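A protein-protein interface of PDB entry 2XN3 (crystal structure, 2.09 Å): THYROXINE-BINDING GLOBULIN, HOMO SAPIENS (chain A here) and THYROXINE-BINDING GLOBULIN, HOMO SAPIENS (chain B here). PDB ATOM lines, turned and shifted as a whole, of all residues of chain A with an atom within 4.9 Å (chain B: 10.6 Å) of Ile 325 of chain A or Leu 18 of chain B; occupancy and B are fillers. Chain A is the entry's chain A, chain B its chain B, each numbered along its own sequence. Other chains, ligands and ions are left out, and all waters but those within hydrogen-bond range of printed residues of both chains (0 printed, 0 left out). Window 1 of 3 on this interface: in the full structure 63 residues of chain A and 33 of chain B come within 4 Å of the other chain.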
ATOM      1  N   PHE A  35      31.646 -29.851  23.499  1.00  0.00           N
ATOM      2  CA  PHE A  35      32.493 -29.955  22.312  1.00  0.00           C
ATOM      3  C   PHE A  35      33.890 -30.544  22.640  1.00  0.00           C
ATOM      4  O   PHE A  35      34.650 -30.011  23.466  1.00  0.00           O
ATOM      5  CB  PHE A  35      32.611 -28.609  21.573  1.00  0.00           C
ATOM      6  CG  PHE A  35      33.216 -28.747  20.222  1.00  0.00           C
ATOM      7  CD1 PHE A  35      32.480 -29.276  19.172  1.00  0.00           C
ATOM      8  CD2 PHE A  35      34.550 -28.435  20.014  1.00  0.00           C
ATOM      9  CE1 PHE A  35      33.056 -29.478  17.950  1.00  0.00           C
ATOM     10  CE2 PHE A  35      35.125 -28.613  18.785  1.00  0.00           C
ATOM     11  CZ  PHE A  35      34.382 -29.160  17.749  1.00  0.00           C
ATOM     12  N   TRP A 178      33.014 -26.581   2.963  1.00  0.00           N
ATOM     13  CA  TRP A 178      31.806 -27.307   2.599  1.00  0.00           C
ATOM     14  C   TRP A 178      31.892 -27.688   1.134  1.00  0.00           C
ATOM     15  O   TRP A 178      32.356 -26.891   0.335  1.00  0.00           O
ATOM     16  CB  TRP A 178      30.577 -26.417   2.758  1.00  0.00           C
ATOM     17  CG  TRP A 178      30.359 -25.903   4.127  1.00  0.00           C
ATOM     18  CD1 TRP A 178      30.280 -24.611   4.502  1.00  0.00           C
ATOM     19  CD2 TRP A 178      30.158 -26.681   5.290  1.00  0.00           C
ATOM     20  NE1 TRP A 178      30.058 -24.522   5.848  1.00  0.00           N
ATOM     21  CE2 TRP A 178      29.981 -25.782   6.363  1.00  0.00           C
ATOM     22  CE3 TRP A 178      30.110 -28.055   5.542  1.00  0.00           C
ATOM     23  CZ2 TRP A 178      29.755 -26.212   7.661  1.00  0.00           C
ATOM     24  CZ3 TRP A 178      29.913 -28.480   6.833  1.00  0.00           C
ATOM     25  CH2 TRP A 178      29.739 -27.563   7.879  1.00  0.00           C
ATOM     26  N   MET A 206      22.609 -19.099   8.187  1.00  0.00           N
ATOM     27  CA  MET A 206      22.984 -19.306   6.789  1.00  0.00           C
ATOM     28  C   MET A 206      21.848 -20.072   6.126  1.00  0.00           C
ATOM     29  O   MET A 206      21.114 -20.773   6.789  1.00  0.00           O
ATOM     30  CB  MET A 206      24.315 -20.063   6.684  1.00  0.00           C
ATOM     31  CG  MET A 206      25.463 -19.373   7.450  1.00  0.00           C
ATOM     32  SD  MET A 206      26.991 -20.265   7.390  1.00  0.00           S
ATOM     33  CE  MET A 206      26.584 -21.875   8.131  1.00  0.00           C
ATOM     34  N   ALA A 235      30.164 -33.454   8.045  1.00  0.00           N
ATOM     35  CA  ALA A 235      29.494 -33.055   9.280  1.00  0.00           C
ATOM     36  C   ALA A 235      28.100 -33.691   9.322  1.00  0.00           C
ATOM     37  O   ALA A 235      27.399 -33.683   8.316  1.00  0.00           O
ATOM     38  CB  ALA A 235      29.374 -31.529   9.349  1.00  0.00           C
ATOM     39  N   LEU A 236      27.712 -34.238  10.476  1.00  0.00           N
ATOM     40  CA  LEU A 236      26.344 -34.682  10.715  1.00  0.00           C
ATOM     41  C   LEU A 236      25.746 -33.745  11.743  1.00  0.00           C
ATOM     42  O   LEU A 236      26.328 -33.528  12.839  1.00  0.00           O
ATOM     43  CB  LEU A 236      26.271 -36.114  11.291  1.00  0.00           C
ATOM     44  CG  LEU A 236      26.387 -37.375  10.441  1.00  0.00           C
ATOM     45  CD1 LEU A 236      25.981 -38.566  11.290  1.00  0.00           C
ATOM     46  CD2 LEU A 236      25.543 -37.328   9.149  1.00  0.00           C
ATOM     47  N   PHE A 237      24.593 -33.193  11.395  1.00  0.00           N
ATOM     48  CA  PHE A 237      23.789 -32.417  12.318  1.00  0.00           C
ATOM     49  C   PHE A 237      22.631 -33.306  12.752  1.00  0.00           C
ATOM     50  O   PHE A 237      21.954 -33.924  11.920  1.00  0.00           O
ATOM     51  CB  PHE A 237      23.270 -31.151  11.633  1.00  0.00           C
ATOM     52  CG  PHE A 237      24.360 -30.171  11.259  1.00  0.00           C
ATOM     53  CD1 PHE A 237      25.146 -30.392  10.161  1.00  0.00           C
ATOM     54  CD2 PHE A 237      24.588 -29.035  12.012  1.00  0.00           C
ATOM     55  CE1 PHE A 237      26.159 -29.496   9.806  1.00  0.00           C
ATOM     56  CE2 PHE A 237      25.593 -28.117  11.652  1.00  0.00           C
ATOM     57  CZ  PHE A 237      26.375 -28.361  10.556  1.00  0.00           C
ATOM     58  N   VAL A 273      21.235 -23.057   8.455  1.00  0.00           N
ATOM     59  CA  VAL A 273      22.250 -23.455   9.451  1.00  0.00           C
ATOM     60  C   VAL A 273      22.885 -22.243  10.132  1.00  0.00           C
ATOM     61  O   VAL A 273      23.291 -21.305   9.471  1.00  0.00           O
ATOM     62  CB  VAL A 273      23.353 -24.304   8.801  1.00  0.00           C
ATOM     63  CG1 VAL A 273      24.485 -24.628   9.803  1.00  0.00           C
ATOM     64  CG2 VAL A 273      22.760 -25.584   8.251  1.00  0.00           C
ATOM     65  N   PRO A 274      23.002 -22.263  11.463  1.00  0.00           N
ATOM     66  CA  PRO A 274      23.610 -21.117  12.133  1.00  0.00           C
ATOM     67  C   PRO A 274      25.103 -20.969  11.869  1.00  0.00           C
ATOM     68  O   PRO A 274      25.805 -21.954  11.718  1.00  0.00           O
ATOM     69  CB  PRO A 274      23.363 -21.401  13.609  1.00  0.00           C
ATOM     70  CG  PRO A 274      23.160 -22.852  13.681  1.00  0.00           C
ATOM     71  CD  PRO A 274      22.587 -23.297  12.408  1.00  0.00           C
ATOM     72  N   LYS A 275      25.558 -19.726  11.826  1.00  0.00           N
ATOM     73  CA  LYS A 275      26.969 -19.389  11.743  1.00  0.00           C
ATOM     74  C   LYS A 275      27.382 -19.046  13.164  1.00  0.00           C
ATOM     75  O   LYS A 275      26.746 -18.218  13.798  1.00  0.00           O
ATOM     76  CB  LYS A 275      27.175 -18.179  10.809  1.00  0.00           C
ATOM     77  CG  LYS A 275      28.591 -17.608  10.744  1.00  0.00           C
ATOM     78  CD  LYS A 275      28.641 -16.323   9.866  1.00  0.00           C
ATOM     79  CE  LYS A 275      30.065 -15.899   9.564  1.00  0.00           C
ATOM     80  NZ  LYS A 275      30.125 -14.876   8.498  1.00  0.00           N
ATOM     81  N   PHE A 276      28.428 -19.691  13.670  1.00  0.00           N
ATOM     82  CA  PHE A 276      28.746 -19.594  15.099  1.00  0.00           C
ATOM     83  C   PHE A 276      30.096 -20.231  15.473  1.00  0.00           C
ATOM     84  O   PHE A 276      30.714 -20.952  14.693  1.00  0.00           O
ATOM     85  CB  PHE A 276      27.643 -20.270  15.935  1.00  0.00           C
ATOM     86  CG  PHE A 276      27.691 -21.769  15.891  1.00  0.00           C
ATOM     87  CD1 PHE A 276      28.226 -22.493  16.947  1.00  0.00           C
ATOM     88  CD2 PHE A 276      27.230 -22.455  14.780  1.00  0.00           C
ATOM     89  CE1 PHE A 276      28.292 -23.872  16.898  1.00  0.00           C
ATOM     90  CE2 PHE A 276      27.286 -23.839  14.721  1.00  0.00           C
ATOM     91  CZ  PHE A 276      27.830 -24.556  15.769  1.00  0.00           C
ATOM     92  N   LEU A 323      35.427 -24.741  17.999  1.00  0.00           N
ATOM     93  CA  LEU A 323      34.716 -24.960  16.739  1.00  0.00           C
ATOM     94  C   LEU A 323      34.269 -23.649  16.140  1.00  0.00           C
ATOM     95  O   LEU A 323      33.737 -22.806  16.837  1.00  0.00           O
ATOM     96  CB  LEU A 323      33.459 -25.787  16.994  1.00  0.00           C
ATOM     97  CG  LEU A 323      32.478 -25.884  15.823  1.00  0.00           C
ATOM     98  CD1 LEU A 323      33.146 -26.686  14.715  1.00  0.00           C
ATOM     99  CD2 LEU A 323      31.148 -26.560  16.282  1.00  0.00           C
ATOM    100  N   HIS A 324      34.443 -23.499  14.838  1.00  0.00           N
ATOM    101  CA  HIS A 324      33.833 -22.396  14.121  1.00  0.00           C
ATOM    102  C   HIS A 324      33.195 -22.896  12.862  1.00  0.00           C
ATOM    103  O   HIS A 324      33.868 -23.542  12.046  1.00  0.00           O
ATOM    104  CB  HIS A 324      34.847 -21.317  13.730  1.00  0.00           C
ATOM    105  CG  HIS A 324      34.248 -20.240  12.870  1.00  0.00           C
ATOM    106  ND1 HIS A 324      33.444 -19.240  13.381  1.00  0.00           N
ATOM    107  CD2 HIS A 324      34.256 -20.066  11.529  1.00  0.00           C
ATOM    108  CE1 HIS A 324      33.019 -18.475  12.392  1.00  0.00           C
ATOM    109  NE2 HIS A 324      33.504 -18.950  11.259  1.00  0.00           N
ATOM    110  N   ILE A 325      31.926 -22.542  12.671  1.00  0.00           N
ATOM    111  CA  ILE A 325      31.207 -22.879  11.441  1.00  0.00           C
ATOM    112  C   ILE A 325      30.713 -21.590  10.784  1.00  0.00           C
ATOM    113  O   ILE A 325      30.056 -20.759  11.423  1.00  0.00           O
ATOM    114  CB  ILE A 325      30.022 -23.857  11.734  1.00  0.00           C
ATOM    115  CG1 ILE A 325      30.585 -25.245  12.024  1.00  0.00           C
ATOM    116  CG2 ILE A 325      29.026 -23.870  10.602  1.00  0.00           C
ATOM    117  CD1 ILE A 325      29.600 -26.294  12.446  1.00  0.00           C
ATOM    118  N   GLY A 326      31.032 -21.447   9.499  1.00  0.00           N
ATOM    119  CA  GLY A 326      30.629 -20.313   8.706  1.00  0.00           C
ATOM    120  C   GLY A 326      30.244 -20.729   7.303  1.00  0.00           C
ATOM    121  O   GLY A 326      30.039 -21.936   7.002  1.00  0.00           O
ATOM    122  N   GLU A 327      30.097 -19.728   6.449  1.00  0.00           N
ATOM    123  CA  GLU A 327      29.627 -19.946   5.086  1.00  0.00           C
ATOM    124  C   GLU A 327      30.582 -20.782   4.262  1.00  0.00           C
ATOM    125  O   GLU A 327      30.143 -21.485   3.357  1.00  0.00           O
ATOM    126  CB  GLU A 327      29.404 -18.608   4.353  1.00  0.00           C
ATOM    127  CG  GLU A 327      28.186 -17.881   4.788  1.00  0.00           C
ATOM    128  CD  GLU A 327      28.417 -16.848   5.882  1.00  0.00           C
ATOM    129  OE1 GLU A 327      29.571 -16.669   6.388  1.00  0.00           O
ATOM    130  OE2 GLU A 327      27.405 -16.193   6.203  1.00  0.00           O
ATOM    131  N   GLY A 329      33.038 -23.054   5.369  1.00  0.00           N
ATOM    132  CA  GLY A 329      33.305 -24.395   5.879  1.00  0.00           C
ATOM    133  C   GLY A 329      33.377 -24.441   7.423  1.00  0.00           C
ATOM    134  O   GLY A 329      32.630 -23.746   8.107  1.00  0.00           O
ATOM    135  N   THR A 330      34.294 -25.240   7.951  1.00  0.00           N
ATOM    136  CA  THR A 330      34.465 -25.445   9.395  1.00  0.00           C
ATOM    137  C   THR A 330      35.942 -25.385   9.733  1.00  0.00           C
ATOM    138  O   THR A 330      36.773 -25.825   8.949  1.00  0.00           O
ATOM    139  CB  THR A 330      33.880 -26.817   9.816  1.00  0.00           C
ATOM    140  OG1 THR A 330      32.500 -26.858   9.456  1.00  0.00           O
ATOM    141  CG2 THR A 330      34.031 -27.094  11.340  1.00  0.00           C
ATOM    142  N   ILE B  12      18.032 -25.568  11.489  1.00  0.00           N
ATOM    143  CA  ILE B  12      18.814 -25.884  12.668  1.00  0.00           C
ATOM    144  C   ILE B  12      18.688 -24.677  13.582  1.00  0.00           C
ATOM    145  O   ILE B  12      19.567 -23.792  13.591  1.00  0.00           O
ATOM    146  CB  ILE B  12      20.295 -26.189  12.347  1.00  0.00           C
ATOM    147  CG1 ILE B  12      20.413 -27.205  11.195  1.00  0.00           C
ATOM    148  CG2 ILE B  12      20.971 -26.752  13.598  1.00  0.00           C
ATOM    149  CD1 ILE B  12      19.804 -28.557  11.516  1.00  0.00           C
ATOM    150  N   ARG B  14      17.316 -24.943  16.988  1.00  0.00           N
ATOM    151  CA  ARG B  14      17.287 -25.299  18.385  1.00  0.00           C
ATOM    152  C   ARG B  14      18.397 -26.302  18.621  1.00  0.00           C
ATOM    153  O   ARG B  14      19.117 -26.668  17.683  1.00  0.00           O
ATOM    154  CB  ARG B  14      15.900 -25.817  18.806  1.00  0.00           C
ATOM    155  CG  ARG B  14      15.310 -26.875  17.912  1.00  0.00           C
ATOM    156  CD  ARG B  14      13.951 -27.391  18.452  1.00  0.00           C
ATOM    157  NE  ARG B  14      13.660 -28.626  17.740  1.00  0.00           N
ATOM    158  CZ  ARG B  14      13.308 -28.670  16.461  1.00  0.00           C
ATOM    159  NH1 ARG B  14      13.138 -27.546  15.769  1.00  0.00           N
ATOM    160  NH2 ARG B  14      13.101 -29.829  15.869  1.00  0.00           N
ATOM    161  N   SER B  15      18.559 -26.730  19.864  1.00  0.00           N
ATOM    162  CA  SER B  15      19.686 -27.569  20.251  1.00  0.00           C
ATOM    163  C   SER B  15      19.893 -28.760  19.343  1.00  0.00           C
ATOM    164  O   SER B  15      18.957 -29.495  19.068  1.00  0.00           O
ATOM    165  CB  SER B  15      19.512 -28.086  21.668  1.00  0.00           C
ATOM    166  OG  SER B  15      19.483 -27.005  22.555  1.00  0.00           O
ATOM    167  N   PHE B  16      21.141 -28.975  18.940  1.00  0.00           N
ATOM    168  CA  PHE B  16      21.482 -30.063  18.052  1.00  0.00           C
ATOM    169  C   PHE B  16      22.789 -30.709  18.467  1.00  0.00           C
ATOM    170  O   PHE B  16      23.585 -30.093  19.192  1.00  0.00           O
ATOM    171  CB  PHE B  16      21.531 -29.572  16.597  1.00  0.00           C
ATOM    172  CG  PHE B  16      22.574 -28.532  16.321  1.00  0.00           C
ATOM    173  CD1 PHE B  16      22.305 -27.192  16.529  1.00  0.00           C
ATOM    174  CD2 PHE B  16      23.834 -28.897  15.860  1.00  0.00           C
ATOM    175  CE1 PHE B  16      23.264 -26.226  16.253  1.00  0.00           C
ATOM    176  CE2 PHE B  16      24.806 -27.937  15.586  1.00  0.00           C
ATOM    177  CZ  PHE B  16      24.511 -26.603  15.779  1.00  0.00           C
ATOM    178  N   MET B  17      22.971 -31.976  18.078  1.00  0.00           N
ATOM    179  CA  MET B  17      24.271 -32.639  18.189  1.00  0.00           C
ATOM    180  C   MET B  17      24.991 -32.463  16.855  1.00  0.00           C
ATOM    181  O   MET B  17      24.352 -32.398  15.798  1.00  0.00           O
ATOM    182  CB  MET B  17      24.115 -34.122  18.587  1.00  0.00           C
ATOM    183  CG  MET B  17      23.768 -34.309  20.077  1.00  0.00           C
ATOM    184  SD  MET B  17      23.628 -36.038  20.597  1.00  0.00           S
ATOM    185  CE  MET B  17      25.324 -36.515  20.250  1.00  0.00           C
ATOM    186  N   LEU B  18      26.316 -32.322  16.927  1.00  0.00           N
ATOM    187  CA  LEU B  18      27.203 -32.185  15.761  1.00  0.00           C
ATOM    188  C   LEU B  18      28.266 -33.283  15.834  1.00  0.00           C
ATOM    189  O   LEU B  18      28.821 -33.560  16.914  1.00  0.00           O
ATOM    190  CB  LEU B  18      27.886 -30.805  15.804  1.00  0.00           C
ATOM    191  CG  LEU B  18      28.856 -30.432  14.701  1.00  0.00           C
ATOM    192  CD1 LEU B  18      28.176 -30.394  13.330  1.00  0.00           C
ATOM    193  CD2 LEU B  18      29.563 -29.099  15.001  1.00  0.00           C
ATOM    194  N   LEU B  19      28.537 -33.929  14.706  1.00  0.00           N
ATOM    195  CA  LEU B  19      29.653 -34.847  14.583  1.00  0.00           C
ATOM    196  C   LEU B  19      30.465 -34.431  13.372  1.00  0.00           C
ATOM    197  O   LEU B  19      29.914 -34.042  12.338  1.00  0.00           O
ATOM    198  CB  LEU B  19      29.179 -36.293  14.422  1.00  0.00           C
ATOM    199  CG  LEU B  19      28.358 -36.893  15.569  1.00  0.00           C
ATOM    200  CD1 LEU B  19      26.892 -36.493  15.470  1.00  0.00           C
ATOM    201  CD2 LEU B  19      28.475 -38.452  15.593  1.00  0.00           C
ATOM    202  N   ILE B  20      31.780 -34.481  13.497  1.00  0.00           N
ATOM    203  CA  ILE B  20      32.652 -34.272  12.355  1.00  0.00           C
ATOM    204  C   ILE B  20      33.468 -35.538  12.164  1.00  0.00           C
ATOM    205  O   ILE B  20      34.192 -35.963  13.080  1.00  0.00           O
ATOM    206  CB  ILE B  20      33.575 -33.071  12.545  1.00  0.00           C
ATOM    207  CG1 ILE B  20      32.741 -31.789  12.632  1.00  0.00           C
ATOM    208  CG2 ILE B  20      34.581 -32.998  11.387  1.00  0.00           C
ATOM    209  CD1 ILE B  20      33.560 -30.551  13.141  1.00  0.00           C
ATOM    210  N   LEU B  21      33.281 -36.155  10.999  1.00  0.00           N
ATOM    211  CA  LEU B  21      33.756 -37.504  10.728  1.00  0.00           C
ATOM    212  C   LEU B  21      34.752 -37.451   9.579  1.00  0.00           C
ATOM    213  O   LEU B  21      34.550 -36.713   8.618  1.00  0.00           O
ATOM    214  CB  LEU B  21      32.573 -38.438  10.365  1.00  0.00           C
ATOM    215  CG  LEU B  21      31.340 -38.412  11.318  1.00  0.00           C
ATOM    216  CD1 LEU B  21      30.166 -39.188  10.750  1.00  0.00           C
ATOM    217  CD2 LEU B  21      31.666 -38.956  12.679  1.00  0.00           C
ATOM    218  N   SER B  27      36.560 -42.120  11.427  1.00  0.00           N
ATOM    219  CA  SER B  27      36.884 -41.553  12.745  1.00  0.00           C
ATOM    220  C   SER B  27      35.921 -40.414  13.095  1.00  0.00           C
ATOM    221  O   SER B  27      35.527 -39.641  12.233  1.00  0.00           O
ATOM    222  CB  SER B  27      38.320 -41.001  12.790  1.00  0.00           C
ATOM    223  OG  SER B  27      39.297 -42.016  12.783  1.00  0.00           O
ATOM    224  N   ILE B  28      35.569 -40.300  14.365  1.00  0.00           N
ATOM    225  CA  ILE B  28      34.890 -39.123  14.848  1.00  0.00           C
ATOM    226  C   ILE B  28      35.960 -38.170  15.298  1.00  0.00           C
ATOM    227  O   ILE B  28      36.578 -38.358  16.369  1.00  0.00           O
ATOM    228  CB  ILE B  28      33.935 -39.409  16.007  1.00  0.00           C
ATOM    229  CG1 ILE B  28      32.928 -40.503  15.631  1.00  0.00           C
ATOM    230  CG2 ILE B  28      33.199 -38.131  16.376  1.00  0.00           C
ATOM    231  CD1 ILE B  28      31.951 -40.818  16.755  1.00  0.00           C
ATOM    232  N   LEU B  29      36.207 -37.161  14.469  1.00  0.00           N
ATOM    233  CA  LEU B  29      37.196 -36.141  14.778  1.00  0.00           C
ATOM    234  C   LEU B  29      36.716 -35.233  15.918  1.00  0.00           C
ATOM    235  O   LEU B  29      37.487 -34.902  16.825  1.00  0.00           O
ATOM    236  CB  LEU B  29      37.520 -35.302  13.533  1.00  0.00           C
ATOM    237  CG  LEU B  29      38.015 -36.071  12.304  1.00  0.00           C
ATOM    238  CD1 LEU B  29      38.297 -35.097  11.139  1.00  0.00           C
ATOM    239  CD2 LEU B  29      39.258 -36.947  12.593  1.00  0.00           C
ATOM    240  N   PHE B  30      35.443 -34.838  15.859  1.00  0.00           N
ATOM    241  CA  PHE B  30      34.842 -33.960  16.859  1.00  0.00           C
ATOM    242  C   PHE B  30      33.409 -34.366  17.091  1.00  0.00           C
ATOM    243  O   PHE B  30      32.720 -34.810  16.164  1.00  0.00           O
ATOM    244  CB  PHE B  30      34.866 -32.501  16.398  1.00  0.00           C
ATOM    245  CG  PHE B  30      36.238 -31.980  16.200  1.00  0.00           C
ATOM    246  CD1 PHE B  30      36.953 -31.467  17.265  1.00  0.00           C
ATOM    247  CD2 PHE B  30      36.821 -32.031  14.964  1.00  0.00           C
ATOM    248  CE1 PHE B  30      38.232 -31.009  17.086  1.00  0.00           C
ATOM    249  CE2 PHE B  30      38.106 -31.599  14.787  1.00  0.00           C
ATOM    250  CZ  PHE B  30      38.809 -31.091  15.846  1.00  0.00           C
ATOM    251  N   LEU B  31      32.964 -34.147  18.314  1.00  0.00           N
ATOM    252  CA  LEU B  31      31.630 -34.506  18.760  1.00  0.00           C
ATOM    253  C   LEU B  31      31.144 -33.432  19.725  1.00  0.00           C
ATOM    254  O   LEU B  31      31.890 -32.984  20.611  1.00  0.00           O
ATOM    255  CB  LEU B  31      31.656 -35.857  19.461  1.00  0.00           C
ATOM    256  CG  LEU B  31      30.374 -36.349  20.154  1.00  0.00           C
ATOM    257  CD1 LEU B  31      29.209 -36.444  19.172  1.00  0.00           C
ATOM    258  CD2 LEU B  31      30.648 -37.707  20.775  1.00  0.00           C
ATOM    259  N   GLY B  32      29.889 -33.032  19.570  1.00  0.00           N
ATOM    260  CA  GLY B  32      29.337 -32.041  20.468  1.00  0.00           C
ATOM    261  C   GLY B  32      27.837 -31.847  20.437  1.00  0.00           C
ATOM    262  O   GLY B  32      27.112 -32.452  19.654  1.00  0.00           O
ATOM    263  N   LYS B  33      27.389 -30.994  21.347  1.00  0.00           N
ATOM    264  CA  LYS B  33      26.024 -30.539  21.363  1.00  0.00           C
ATOM    265  C   LYS B  33      26.043 -29.043  21.483  1.00  0.00           C
ATOM    266  O   LYS B  33      26.673 -28.491  22.397  1.00  0.00           O
ATOM    267  CB  LYS B  33      25.279 -31.167  22.530  1.00  0.00           C
ATOM    268  CG  LYS B  33      23.915 -30.544  22.785  1.00  0.00           C
ATOM    269  CD  LYS B  33      23.110 -31.347  23.837  1.00  0.00           C
ATOM    270  CE  LYS B  33      23.796 -31.379  25.192  1.00  0.00           C
ATOM    271  NZ  LYS B  33      22.850 -31.881  26.236  1.00  0.00           N
ATOM    272  N   VAL B  34      25.360 -28.386  20.553  1.00  0.00           N
ATOM    273  CA  VAL B  34      25.171 -26.948  20.621  1.00  0.00           C
ATOM    274  C   VAL B  34      23.817 -26.668  21.237  1.00  0.00           C
ATOM    275  O   VAL B  34      22.792 -26.876  20.599  1.00  0.00           O
ATOM    276  CB  VAL B  34      25.251 -26.286  19.263  1.00  0.00           C
ATOM    277  CG1 VAL B  34      25.040 -24.801  19.424  1.00  0.00           C
ATOM    278  CG2 VAL B  34      26.616 -26.600  18.584  1.00  0.00           C
ATOM    279  N   VAL B  35      23.839 -26.209  22.488  1.00  0.00           N
ATOM    280  CA  VAL B  35      22.663 -25.776  23.220  1.00  0.00           C
ATOM    281  C   VAL B  35      22.440 -24.280  23.015  1.00  0.00           C
ATOM    282  O   VAL B  35      21.315 -23.852  22.769  1.00  0.00           O
ATOM    283  CB  VAL B  35      22.785 -26.135  24.727  1.00  0.00           C
ATOM    284  CG1 VAL B  35      21.667 -25.508  25.540  1.00  0.00           C
ATOM    285  CG2 VAL B  35      22.775 -27.637  24.903  1.00  0.00           C
ATOM    286  N   PRO B  37      24.468 -21.357  20.750  1.00  0.00           N
ATOM    287  CA  PRO B  37      25.593 -21.036  19.856  1.00  0.00           C
ATOM    288  C   PRO B  37      26.240 -19.658  20.061  1.00  0.00           C
ATOM    289  O   PRO B  37      27.235 -19.368  19.412  1.00  0.00           O
ATOM    290  CB  PRO B  37      24.982 -21.150  18.461  1.00  0.00           C
ATOM    291  CG  PRO B  37      23.487 -21.054  18.655  1.00  0.00           C
ATOM    292  CD  PRO B  37      23.168 -21.409  20.048  1.00  0.00           C
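CD1 of Phe 30 of chain B touches CZ of Phe 35 of chain A, 3.5 Å away.
Phe 35 of chain A touches Leu 31 of chain B.
CA of Ala 235 of chain A touches O of Leu 19 of chain B, 3.2 Å away.
Leu 236 of chain A touches Met 17 of chain B.
Leu 18 of chain B touches Leu 236 of chain A (CA to O, 3.3 Å).
Met 17 of chain B touches Phe 237 of chain A.
CE2 of Phe 237 of chain A touches CD1 of Leu 18 of chain B, 3.8 Å away.
Phe 16 of chain B touches Phe 276 of chain A (CZ to CZ, 3.9 Å).
CG2 of Val 34 of chain B touches CE1 of Phe 276 of chain A, at 3.6 Å.
CD1 of Ile 20 of chain B touches CG2 of Thr 330 of chain A (3.9 Å).
Printed residues of chain A that touch a printed residue of chain B: Phe 35, Ala 235, Leu 236, Phe 237, Pro 274, Phe 276, Leu 323, Ile 325 and Thr 330.
Hydrophobic or aromatic side chains of chain A that line the printed part of chain B: Phe 35, Ala 235, Phe 237, Pro 274, Phe 276, Leu 323 and Ile 325.
Hydrophobic or aromatic side chains of chain B that line the printed part of chain A: Ile 12, Phe 16, Leu 18, Ile 20, Phe 30, Val 34 and Pro 37.
Among the printed residues, 16 pairs touch across the chains.
A ring nitrogen (ND1) of His 324 of chain A lies within hydrogen-bond range of the backbone carbonyl oxygen of Phe 276 of chain A, at 3.5 Å.
O of Phe 276 of chain A sits at hydrogen-bond distance from N of Ile 325 of chain A (2.8 Å).
The backbone carbonyl oxygen of Phe 16 of chain B lies within hydrogen-bond range of the backbone NH of Val 34 of chain B, at 2.8 Å.
O of Ile 20 of chain B sits at hydrogen-bond distance from N of Leu 29 of chain B (2.7 Å).
The backbone carbonyl oxygen (O) of Phe 30 of chain B is in hydrogen-bond range of the backbone NH (N) of Ile 20 of chain B.
The backbone NH of Leu 18 of chain B sits at hydrogen-bond distance from the backbone carbonyl oxygen of Gly 32 of chain B (2.8 Å).
Of the printed residues of chain B, Leu 236 of chain A touches Met 17 (3.7 Å), Leu 18 (3.3 Å) and Leu 19 (2.9 Å).
Of the printed residues of chain B, Pro 274 of chain A touches Ile 12 (3.3 Å).
Of the printed residues of chain B, Phe 276 of chain A touches Phe 16, Val 34 and Pro 37.
No residue of chain B comes within 4 Å of His 324 of chain A.
Of chain B, only Leu 18 (3.8 Å) comes within 4 Å of Ile 325 of chain A.
No residue of chain B comes within 4 Å of Gly 326 of chain A.
No residue of chain B comes within 4 Å of Gly 329 of chain A.
Of the printed residues of chain A, Phe 16 of chain B touches Phe 237 (3.7 Å) and Phe 276 (3.9 Å).
Of chain A, only Leu 236 (3.3 Å), Phe 237 (3.8 Å), Leu 323 (3.3 Å) and Ile 325 (3.8 Å) come within 4 Å of Leu 18 of chain B.
Ser 27 of chain B touches none of the printed residues of chain A.
The nearest residue of chain B that does not touch Ile 325 of chain A is Ile 20 of chain B (5.9 Å).
The nearest residue of chain A that does not touch Leu 18 of chain B is Ala 235 of chain A (4.3 Å).
The backbone NH of Leu 236 of chain A sits at hydrogen-bond distance from the backbone carbonyl oxygen of Leu 19 of chain B (2.9 Å).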
